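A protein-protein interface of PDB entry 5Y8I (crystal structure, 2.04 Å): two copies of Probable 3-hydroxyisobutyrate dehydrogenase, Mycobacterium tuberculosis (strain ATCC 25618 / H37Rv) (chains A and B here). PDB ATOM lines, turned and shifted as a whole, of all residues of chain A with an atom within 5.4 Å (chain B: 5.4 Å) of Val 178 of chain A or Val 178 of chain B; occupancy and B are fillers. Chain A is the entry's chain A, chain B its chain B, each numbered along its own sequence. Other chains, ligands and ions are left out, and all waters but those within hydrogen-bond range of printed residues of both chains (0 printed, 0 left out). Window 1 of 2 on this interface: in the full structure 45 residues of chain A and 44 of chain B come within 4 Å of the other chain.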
ATOM      1  N   ASN A 173      -4.889  25.434  33.098  1.00  0.00           N
ATOM      2  CA  ASN A 173      -4.936  23.982  33.292  1.00  0.00           C
ATOM      3  C   ASN A 173      -6.283  23.498  33.868  1.00  0.00           C
ATOM      4  O   ASN A 173      -6.690  22.381  33.575  1.00  0.00           O
ATOM      5  CB  ASN A 173      -3.724  23.455  34.086  1.00  0.00           C
ATOM      6  CG  ASN A 173      -2.432  23.473  33.264  1.00  0.00           C
ATOM      7  OD1 ASN A 173      -2.360  24.092  32.184  1.00  0.00           O
ATOM      8  ND2 ASN A 173      -1.400  22.809  33.770  1.00  0.00           N
ATOM      9  N   MET A 174      -6.976  24.343  34.635  1.00  0.00           N
ATOM     10  CA  MET A 174      -8.345  24.031  35.068  1.00  0.00           C
ATOM     11  C   MET A 174      -9.304  23.946  33.864  1.00  0.00           C
ATOM     12  O   MET A 174     -10.164  23.053  33.798  1.00  0.00           O
ATOM     13  CB  MET A 174      -8.862  25.066  36.065  1.00  0.00           C
ATOM     14  CG  MET A 174     -10.235  24.741  36.653  1.00  0.00           C
ATOM     15  SD  MET A 174     -10.746  25.841  37.999  1.00  0.00           S
ATOM     16  CE  MET A 174     -11.008  27.370  37.094  1.00  0.00           C
ATOM     17  N   VAL A 175      -9.160  24.887  32.929  1.00  0.00           N
ATOM     18  CA  VAL A 175      -9.969  24.889  31.705  1.00  0.00           C
ATOM     19  C   VAL A 175      -9.648  23.649  30.862  1.00  0.00           C
ATOM     20  O   VAL A 175     -10.556  23.017  30.326  1.00  0.00           O
ATOM     21  CB  VAL A 175      -9.774  26.197  30.900  1.00  0.00           C
ATOM     22  CG1 VAL A 175     -10.350  26.098  29.485  1.00  0.00           C
ATOM     23  CG2 VAL A 175     -10.425  27.346  31.645  1.00  0.00           C
ATOM     24  N   LEU A 176      -8.363  23.312  30.763  1.00  0.00           N
ATOM     25  CA  LEU A 176      -7.895  22.144  29.998  1.00  0.00           C
ATOM     26  C   LEU A 176      -8.482  20.838  30.520  1.00  0.00           C
ATOM     27  O   LEU A 176      -8.941  20.006  29.743  1.00  0.00           O
ATOM     28  CB  LEU A 176      -6.367  22.069  30.024  1.00  0.00           C
ATOM     29  CG  LEU A 176      -5.686  20.885  29.314  1.00  0.00           C
ATOM     30  CD1 LEU A 176      -6.089  20.815  27.850  1.00  0.00           C
ATOM     31  CD2 LEU A 176      -4.176  20.965  29.452  1.00  0.00           C
ATOM     32  N   ALA A 177      -8.455  20.676  31.841  1.00  0.00           N
ATOM     33  CA  ALA A 177      -9.011  19.508  32.493  1.00  0.00           C
ATOM     34  C   ALA A 177     -10.496  19.348  32.165  1.00  0.00           C
ATOM     35  O   ALA A 177     -10.945  18.249  31.854  1.00  0.00           O
ATOM     36  CB  ALA A 177      -8.807  19.596  33.997  1.00  0.00           C
ATOM     37  N   VAL A 178     -11.242  20.453  32.214  1.00  0.00           N
ATOM     38  CA  VAL A 178     -12.674  20.443  31.895  1.00  0.00           C
ATOM     39  C   VAL A 178     -12.857  20.055  30.427  1.00  0.00           C
ATOM     40  O   VAL A 178     -13.653  19.173  30.119  1.00  0.00           O
ATOM     41  CB  VAL A 178     -13.360  21.790  32.237  1.00  0.00           C
ATOM     42  CG1 VAL A 178     -14.784  21.857  31.680  1.00  0.00           C
ATOM     43  CG2 VAL A 178     -13.389  22.009  33.752  1.00  0.00           C
ATOM     44  N   GLN A 179     -12.086  20.679  29.540  1.00  0.00           N
ATOM     45  CA  GLN A 179     -12.158  20.386  28.113  1.00  0.00           C
ATOM     46  C   GLN A 179     -11.827  18.931  27.781  1.00  0.00           C
ATOM     47  O   GLN A 179     -12.498  18.328  26.936  1.00  0.00           O
ATOM     48  CB  GLN A 179     -11.227  21.291  27.325  1.00  0.00           C
ATOM     49  CG  GLN A 179     -11.665  22.744  27.269  1.00  0.00           C
ATOM     50  CD  GLN A 179     -10.572  23.680  26.808  1.00  0.00           C
ATOM     51  OE1 GLN A 179      -9.385  23.398  26.979  1.00  0.00           O
ATOM     52  NE2 GLN A 179     -10.966  24.821  26.225  1.00  0.00           N
ATOM     53  N   GLN A 180     -10.805  18.373  28.432  1.00  0.00           N
ATOM     54  CA  GLN A 180     -10.408  16.988  28.158  1.00  0.00           C
ATOM     55  C   GLN A 180     -11.502  15.992  28.542  1.00  0.00           C
ATOM     56  O   GLN A 180     -11.692  14.992  27.859  1.00  0.00           O
ATOM     57  CB  GLN A 180      -9.084  16.619  28.827  1.00  0.00           C
ATOM     58  CG  GLN A 180      -8.455  15.353  28.250  1.00  0.00           C
ATOM     59  CD  GLN A 180      -7.878  15.536  26.851  1.00  0.00           C
ATOM     60  OE1 GLN A 180      -6.977  16.349  26.642  1.00  0.00           O
ATOM     61  NE2 GLN A 180      -8.387  14.782  25.887  1.00  0.00           N
ATOM     62  N   ILE A 181     -12.234  16.289  29.612  1.00  0.00           N
ATOM     63  CA  ILE A 181     -13.351  15.455  30.025  1.00  0.00           C
ATOM     64  C   ILE A 181     -14.541  15.653  29.100  1.00  0.00           C
ATOM     65  O   ILE A 181     -15.163  14.676  28.675  1.00  0.00           O
ATOM     66  CB  ILE A 181     -13.748  15.737  31.481  1.00  0.00           C
ATOM     67  CG1 ILE A 181     -12.604  15.312  32.416  1.00  0.00           C
ATOM     68  CG2 ILE A 181     -15.029  14.989  31.837  1.00  0.00           C
ATOM     69  CD1 ILE A 181     -12.648  15.944  33.787  1.00  0.00           C
ATOM     70  N   ALA A 182     -14.859  16.907  28.790  1.00  0.00           N
ATOM     71  CA  ALA A 182     -15.978  17.196  27.888  1.00  0.00           C
ATOM     72  C   ALA A 182     -15.790  16.523  26.524  1.00  0.00           C
ATOM     73  O   ALA A 182     -16.717  15.903  26.001  1.00  0.00           O
ATOM     74  CB  ALA A 182     -16.157  18.697  27.718  1.00  0.00           C
ATOM     75  N   ILE A 183     -14.586  16.641  25.966  1.00  0.00           N
ATOM     76  CA  ILE A 183     -14.246  15.965  24.710  1.00  0.00           C
ATOM     77  C   ILE A 183     -14.448  14.456  24.827  1.00  0.00           C
ATOM     78  O   ILE A 183     -15.003  13.843  23.911  1.00  0.00           O
ATOM     79  CB  ILE A 183     -12.804  16.312  24.240  1.00  0.00           C
ATOM     80  CG1 ILE A 183     -12.773  17.740  23.676  1.00  0.00           C
ATOM     81  CG2 ILE A 183     -12.244  15.316  23.241  1.00  0.00           C
ATOM     82  CD1 ILE A 183     -13.610  18.004  22.435  1.00  0.00           C
ATOM     83  N   GLU A 185     -16.445  12.802  26.944  1.00  0.00           N
ATOM     84  CA  GLU A 185     -17.896  12.574  26.992  1.00  0.00           C
ATOM     85  C   GLU A 185     -18.489  12.600  25.581  1.00  0.00           C
ATOM     86  O   GLU A 185     -19.296  11.741  25.230  1.00  0.00           O
ATOM     87  CB  GLU A 185     -18.606  13.636  27.827  1.00  0.00           C
ATOM     88  CG  GLU A 185     -18.265  13.635  29.309  1.00  0.00           C
ATOM     89  CD  GLU A 185     -18.859  14.838  30.066  1.00  0.00           C
ATOM     90  OE1 GLU A 185     -19.577  15.701  29.484  1.00  0.00           O
ATOM     91  OE2 GLU A 185     -18.596  14.933  31.282  1.00  0.00           O
ATOM     92  N   LEU A 262     -17.720  23.556  37.362  1.00  0.00           N
ATOM     93  CA  LEU A 262     -17.170  22.566  36.433  1.00  0.00           C
ATOM     94  C   LEU A 262     -15.696  22.257  36.718  1.00  0.00           C
ATOM     95  O   LEU A 262     -15.278  21.106  36.624  1.00  0.00           O
ATOM     96  CB  LEU A 262     -17.381  22.987  34.979  1.00  0.00           C
ATOM     97  CG  LEU A 262     -18.837  23.110  34.518  1.00  0.00           C
ATOM     98  CD1 LEU A 262     -18.887  23.356  33.015  1.00  0.00           C
ATOM     99  CD2 LEU A 262     -19.683  21.891  34.886  1.00  0.00           C
ATOM    100  N   GLY A 263     -14.929  23.274  37.092  1.00  0.00           N
ATOM    101  CA  GLY A 263     -13.555  23.079  37.528  1.00  0.00           C
ATOM    102  C   GLY A 263     -13.447  22.160  38.726  1.00  0.00           C
ATOM    103  O   GLY A 263     -12.631  21.235  38.721  1.00  0.00           O
ATOM    104  N   ALA A 266     -14.390  18.635  37.708  1.00  0.00           N
ATOM    105  CA  ALA A 266     -13.243  18.074  37.005  1.00  0.00           C
ATOM    106  C   ALA A 266     -12.171  17.652  37.987  1.00  0.00           C
ATOM    107  O   ALA A 266     -11.556  16.600  37.839  1.00  0.00           O
ATOM    108  CB  ALA A 266     -12.675  19.077  36.006  1.00  0.00           C
ATOM    109  N   ASN B 173     -22.251  21.082  20.494  1.00  0.00           N
ATOM    110  CA  ASN B 173     -22.857  22.147  21.319  1.00  0.00           C
ATOM    111  C   ASN B 173     -22.833  21.843  22.829  1.00  0.00           C
ATOM    112  O   ASN B 173     -22.792  22.765  23.648  1.00  0.00           O
ATOM    113  CB  ASN B 173     -24.275  22.505  20.826  1.00  0.00           C
ATOM    114  CG  ASN B 173     -24.259  23.361  19.552  1.00  0.00           C
ATOM    115  OD1 ASN B 173     -23.221  23.535  18.904  1.00  0.00           O
ATOM    116  ND2 ASN B 173     -25.408  23.897  19.189  1.00  0.00           N
ATOM    117  N   MET B 174     -22.837  20.563  23.192  1.00  0.00           N
ATOM    118  CA  MET B 174     -22.615  20.165  24.580  1.00  0.00           C
ATOM    119  C   MET B 174     -21.208  20.593  25.024  1.00  0.00           C
ATOM    120  O   MET B 174     -21.037  21.205  26.087  1.00  0.00           O
ATOM    121  CB  MET B 174     -22.776  18.648  24.761  1.00  0.00           C
ATOM    122  CG  MET B 174     -22.775  18.211  26.226  1.00  0.00           C
ATOM    123  SD  MET B 174     -23.203  16.480  26.521  1.00  0.00           S
ATOM    124  CE  MET B 174     -21.889  15.607  25.662  1.00  0.00           C
ATOM    125  N   VAL B 175     -20.222  20.277  24.196  1.00  0.00           N
ATOM    126  CA  VAL B 175     -18.835  20.654  24.465  1.00  0.00           C
ATOM    127  C   VAL B 175     -18.729  22.174  24.615  1.00  0.00           C
ATOM    128  O   VAL B 175     -18.170  22.648  25.591  1.00  0.00           O
ATOM    129  CB  VAL B 175     -17.863  20.139  23.394  1.00  0.00           C
ATOM    130  CG1 VAL B 175     -16.456  20.675  23.633  1.00  0.00           C
ATOM    131  CG2 VAL B 175     -17.836  18.631  23.405  1.00  0.00           C
ATOM    132  N   LEU B 176     -19.334  22.904  23.683  1.00  0.00           N
ATOM    133  CA  LEU B 176     -19.364  24.360  23.724  1.00  0.00           C
ATOM    134  C   LEU B 176     -19.921  24.918  25.035  1.00  0.00           C
ATOM    135  O   LEU B 176     -19.318  25.826  25.623  1.00  0.00           O
ATOM    136  CB  LEU B 176     -20.153  24.903  22.549  1.00  0.00           C
ATOM    137  CG  LEU B 176     -20.316  26.426  22.460  1.00  0.00           C
ATOM    138  CD1 LEU B 176     -18.956  27.114  22.320  1.00  0.00           C
ATOM    139  CD2 LEU B 176     -21.233  26.748  21.282  1.00  0.00           C
ATOM    140  N   ALA B 177     -21.045  24.367  25.488  1.00  0.00           N
ATOM    141  CA  ALA B 177     -21.691  24.794  26.734  1.00  0.00           C
ATOM    142  C   ALA B 177     -20.750  24.632  27.914  1.00  0.00           C
ATOM    143  O   ALA B 177     -20.576  25.545  28.716  1.00  0.00           O
ATOM    144  CB  ALA B 177     -22.973  24.009  26.977  1.00  0.00           C
ATOM    145  N   VAL B 178     -20.125  23.473  27.985  1.00  0.00           N
ATOM    146  CA  VAL B 178     -19.144  23.177  29.020  1.00  0.00           C
ATOM    147  C   VAL B 178     -17.956  24.158  28.950  1.00  0.00           C
ATOM    148  O   VAL B 178     -17.543  24.704  29.967  1.00  0.00           O
ATOM    149  CB  VAL B 178     -18.687  21.705  28.894  1.00  0.00           C
ATOM    150  CG1 VAL B 178     -17.462  21.421  29.740  1.00  0.00           C
ATOM    151  CG2 VAL B 178     -19.823  20.758  29.281  1.00  0.00           C
ATOM    152  N   GLN B 179     -17.417  24.374  27.752  1.00  0.00           N
ATOM    153  CA  GLN B 179     -16.314  25.314  27.544  1.00  0.00           C
ATOM    154  C   GLN B 179     -16.669  26.755  27.924  1.00  0.00           C
ATOM    155  O   GLN B 179     -15.836  27.469  28.470  1.00  0.00           O
ATOM    156  CB  GLN B 179     -15.853  25.296  26.078  1.00  0.00           C
ATOM    157  CG  GLN B 179     -15.122  24.030  25.665  1.00  0.00           C
ATOM    158  CD  GLN B 179     -14.966  23.896  24.160  1.00  0.00           C
ATOM    159  OE1 GLN B 179     -15.717  24.492  23.389  1.00  0.00           O
ATOM    160  NE2 GLN B 179     -13.996  23.092  23.733  1.00  0.00           N
ATOM    161  N   GLN B 180     -17.887  27.189  27.611  1.00  0.00           N
ATOM    162  CA  GLN B 180     -18.303  28.568  27.914  1.00  0.00           C
ATOM    163  C   GLN B 180     -18.418  28.784  29.423  1.00  0.00           C
ATOM    164  O   GLN B 180     -18.029  29.838  29.927  1.00  0.00           O
ATOM    165  CB  GLN B 180     -19.615  28.930  27.208  1.00  0.00           C
ATOM    166  CG  GLN B 180     -19.942  30.414  27.168  1.00  0.00           C
ATOM    167  CD  GLN B 180     -18.946  31.207  26.339  1.00  0.00           C
ATOM    168  OE1 GLN B 180     -18.899  31.092  25.110  1.00  0.00           O
ATOM    169  NE2 GLN B 180     -18.120  31.990  27.012  1.00  0.00           N
ATOM    170  N   ILE B 181     -18.922  27.791  30.142  1.00  0.00           N
ATOM    171  CA  ILE B 181     -18.952  27.852  31.614  1.00  0.00           C
ATOM    172  C   ILE B 181     -17.509  27.843  32.185  1.00  0.00           C
ATOM    173  O   ILE B 181     -17.175  28.647  33.067  1.00  0.00           O
ATOM    174  CB  ILE B 181     -19.798  26.708  32.214  1.00  0.00           C
ATOM    175  CG1 ILE B 181     -21.282  26.869  31.824  1.00  0.00           C
ATOM    176  CG2 ILE B 181     -19.676  26.671  33.736  1.00  0.00           C
ATOM    177  CD1 ILE B 181     -22.105  25.599  31.978  1.00  0.00           C
ATOM    178  N   ALA B 182     -16.667  26.952  31.672  1.00  0.00           N
ATOM    179  CA  ALA B 182     -15.296  26.827  32.180  1.00  0.00           C
ATOM    180  C   ALA B 182     -14.478  28.102  31.954  1.00  0.00           C
ATOM    181  O   ALA B 182     -13.705  28.499  32.833  1.00  0.00           O
ATOM    182  CB  ALA B 182     -14.586  25.626  31.572  1.00  0.00           C
ATOM    183  N   ILE B 183     -14.662  28.736  30.794  1.00  0.00           N
ATOM    184  CA  ILE B 183     -13.992  29.998  30.491  1.00  0.00           C
ATOM    185  C   ILE B 183     -14.493  31.092  31.438  1.00  0.00           C
ATOM    186  O   ILE B 183     -13.688  31.850  31.962  1.00  0.00           O
ATOM    187  CB  ILE B 183     -14.131  30.389  29.001  1.00  0.00           C
ATOM    188  CG1 ILE B 183     -13.262  29.462  28.127  1.00  0.00           C
ATOM    189  CG2 ILE B 183     -13.798  31.860  28.750  1.00  0.00           C
ATOM    190  CD1 ILE B 183     -11.764  29.541  28.351  1.00  0.00           C
ATOM    191  N   GLU B 185     -15.647  30.675  34.515  1.00  0.00           N
ATOM    192  CA  GLU B 185     -15.041  30.347  35.807  1.00  0.00           C
ATOM    193  C   GLU B 185     -13.594  30.838  35.917  1.00  0.00           C
ATOM    194  O   GLU B 185     -13.201  31.428  36.940  1.00  0.00           O
ATOM    195  CB  GLU B 185     -15.062  28.828  36.066  1.00  0.00           C
ATOM    196  CG  GLU B 185     -16.446  28.216  36.259  1.00  0.00           C
ATOM    197  CD  GLU B 185     -16.424  26.687  36.376  1.00  0.00           C
ATOM    198  OE1 GLU B 185     -15.331  26.054  36.459  1.00  0.00           O
ATOM    199  OE2 GLU B 185     -17.528  26.096  36.407  1.00  0.00           O
ATOM    200  N   LEU B 262     -19.982  16.286  33.092  1.00  0.00           N
ATOM    201  CA  LEU B 262     -19.870  17.734  32.929  1.00  0.00           C
ATOM    202  C   LEU B 262     -20.929  18.273  31.996  1.00  0.00           C
ATOM    203  O   LEU B 262     -21.449  19.352  32.227  1.00  0.00           O
ATOM    204  CB  LEU B 262     -18.471  18.148  32.467  1.00  0.00           C
ATOM    205  CG  LEU B 262     -17.302  17.747  33.384  1.00  0.00           C
ATOM    206  CD1 LEU B 262     -16.020  18.461  32.957  1.00  0.00           C
ATOM    207  CD2 LEU B 262     -17.607  18.046  34.841  1.00  0.00           C
ATOM    208  N   GLY B 263     -21.263  17.531  30.948  1.00  0.00           N
ATOM    209  CA  GLY B 263     -22.337  17.940  30.027  1.00  0.00           C
ATOM    210  C   GLY B 263     -23.677  18.052  30.739  1.00  0.00           C
ATOM    211  O   GLY B 263     -24.405  19.026  30.548  1.00  0.00           O
ATOM    212  N   ALA B 266     -23.490  21.093  33.076  1.00  0.00           N
ATOM    213  CA  ALA B 266     -23.689  22.252  32.240  1.00  0.00           C
ATOM    214  C   ALA B 266     -25.164  22.426  31.855  1.00  0.00           C
ATOM    215  O   ALA B 266     -25.662  23.546  31.866  1.00  0.00           O
ATOM    216  CB  ALA B 266     -22.806  22.161  31.007  1.00  0.00           C
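The side-chain carboxylate (OE2) of Glu 185 of chain A sits at hydrogen-bond distance from the backbone NH (N) of Leu 262 of chain B, 2.7 Å away.
The backbone NH of Gly 263 of chain B lies within hydrogen-bond range of the side-chain carboxylate of Glu 185 of chain A (2.9 Å).
N of Leu 262 of chain A lies within hydrogen-bond range of OE2 of Glu 185 of chain B (2.7 Å).
The backbone NH of Gly 263 of chain A is in hydrogen-bond range of the side-chain carboxylate of Glu 185 of chain B (2.9 Å).
Val 175 of chain A touches Ile 183 of chain B, but with the chains exchanged Ile 183 of chain A does not touch Val 175 of chain B (4.1 Å).
Val 178 of chain A touches Ala 182 of chain B, and with the chains exchanged Ala 182 of chain A touches Val 178 of chain B.
Val 178 of chain A touches Leu 262 of chain B, and with the chains exchanged Leu 262 of chain A touches Val 178 of chain B.
Glu 185 of chain A touches Leu 262 of chain B, and with the chains exchanged Leu 262 of chain A touches Glu 185 of chain B.
Of chain B, only Val 178 (3.3 Å), Ala 182 (3.8 Å) and Leu 262 (3.8 Å) come within 4 Å of Val 178 of chain A.
Val 178 of chain B touches just these residues of chain A: Val 178, Ala 182 and Leu 262.
Of the printed residues of chain B, Gly 263 of chain A touches Glu 185.
Of the printed residues of chain B, Ile 181 of chain A touches Leu 262 (3.8 Å).
Of the printed residues of chain A, Leu 262 of chain B touches Val 178, Ile 181 and Glu 185.
Printed residues of chain A within 4 Å of Val 175 of chain B: Ala 182 (3.9 Å).
Printed residues of chain A within 4 Å of Ile 181 of chain B: Leu 262 (3.5 Å).
Gln 179 of chain B touches none of the printed residues of chain A.
The nearest residue of chain B that does not touch Val 178 of chain A is Glu 185 of chain B (5.2 Å).
Hydrophobic or aromatic side chains of chain B that line the printed part of chain A: Val 175, Val 178, Ile 181, Ala 182, Ile 183 and Leu 262.
Printed residues of chain A that touch a printed residue of chain B: Val 175, Val 178, Ile 181, Ala 182, Glu 185, Leu 262 and Gly 263.
Among the printed residues, 14 pairs touch across the chains.
Among the printed residues, no Asp or Glu carboxylate lies within 4 Å of a Lys or Arg side-chain nitrogen of the other chain.
CG2 of Val 175 of chain A touches O of Ala 182 of chain B, at 3.7 Å.
Val 175 of chain A touches Ile 183 of chain B.
CG1 of Val 178 of chain B touches CG1 of Val 178 of chain A, at 3.3 Å.
Val 178 of chain A touches Ala 182 of chain B (CG1 to CB, 3.8 Å).
Leu 262 of chain B touches Val 178 of chain A.
Ile 181 of chain A touches Leu 262 of chain B (CG2 to CD1, 3.8 Å).
Ala 182 of chain A touches Val 175 of chain B.
Ala 182 of chain A touches Val 178 of chain B (CB to CG1, 3.6 Å).
CD1 of Leu 262 of chain A touches O of Val 178 of chain B (3.6 Å).
CD1 of Leu 262 of chain A touches CG2 of Ile 181 of chain B (3.5 Å).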
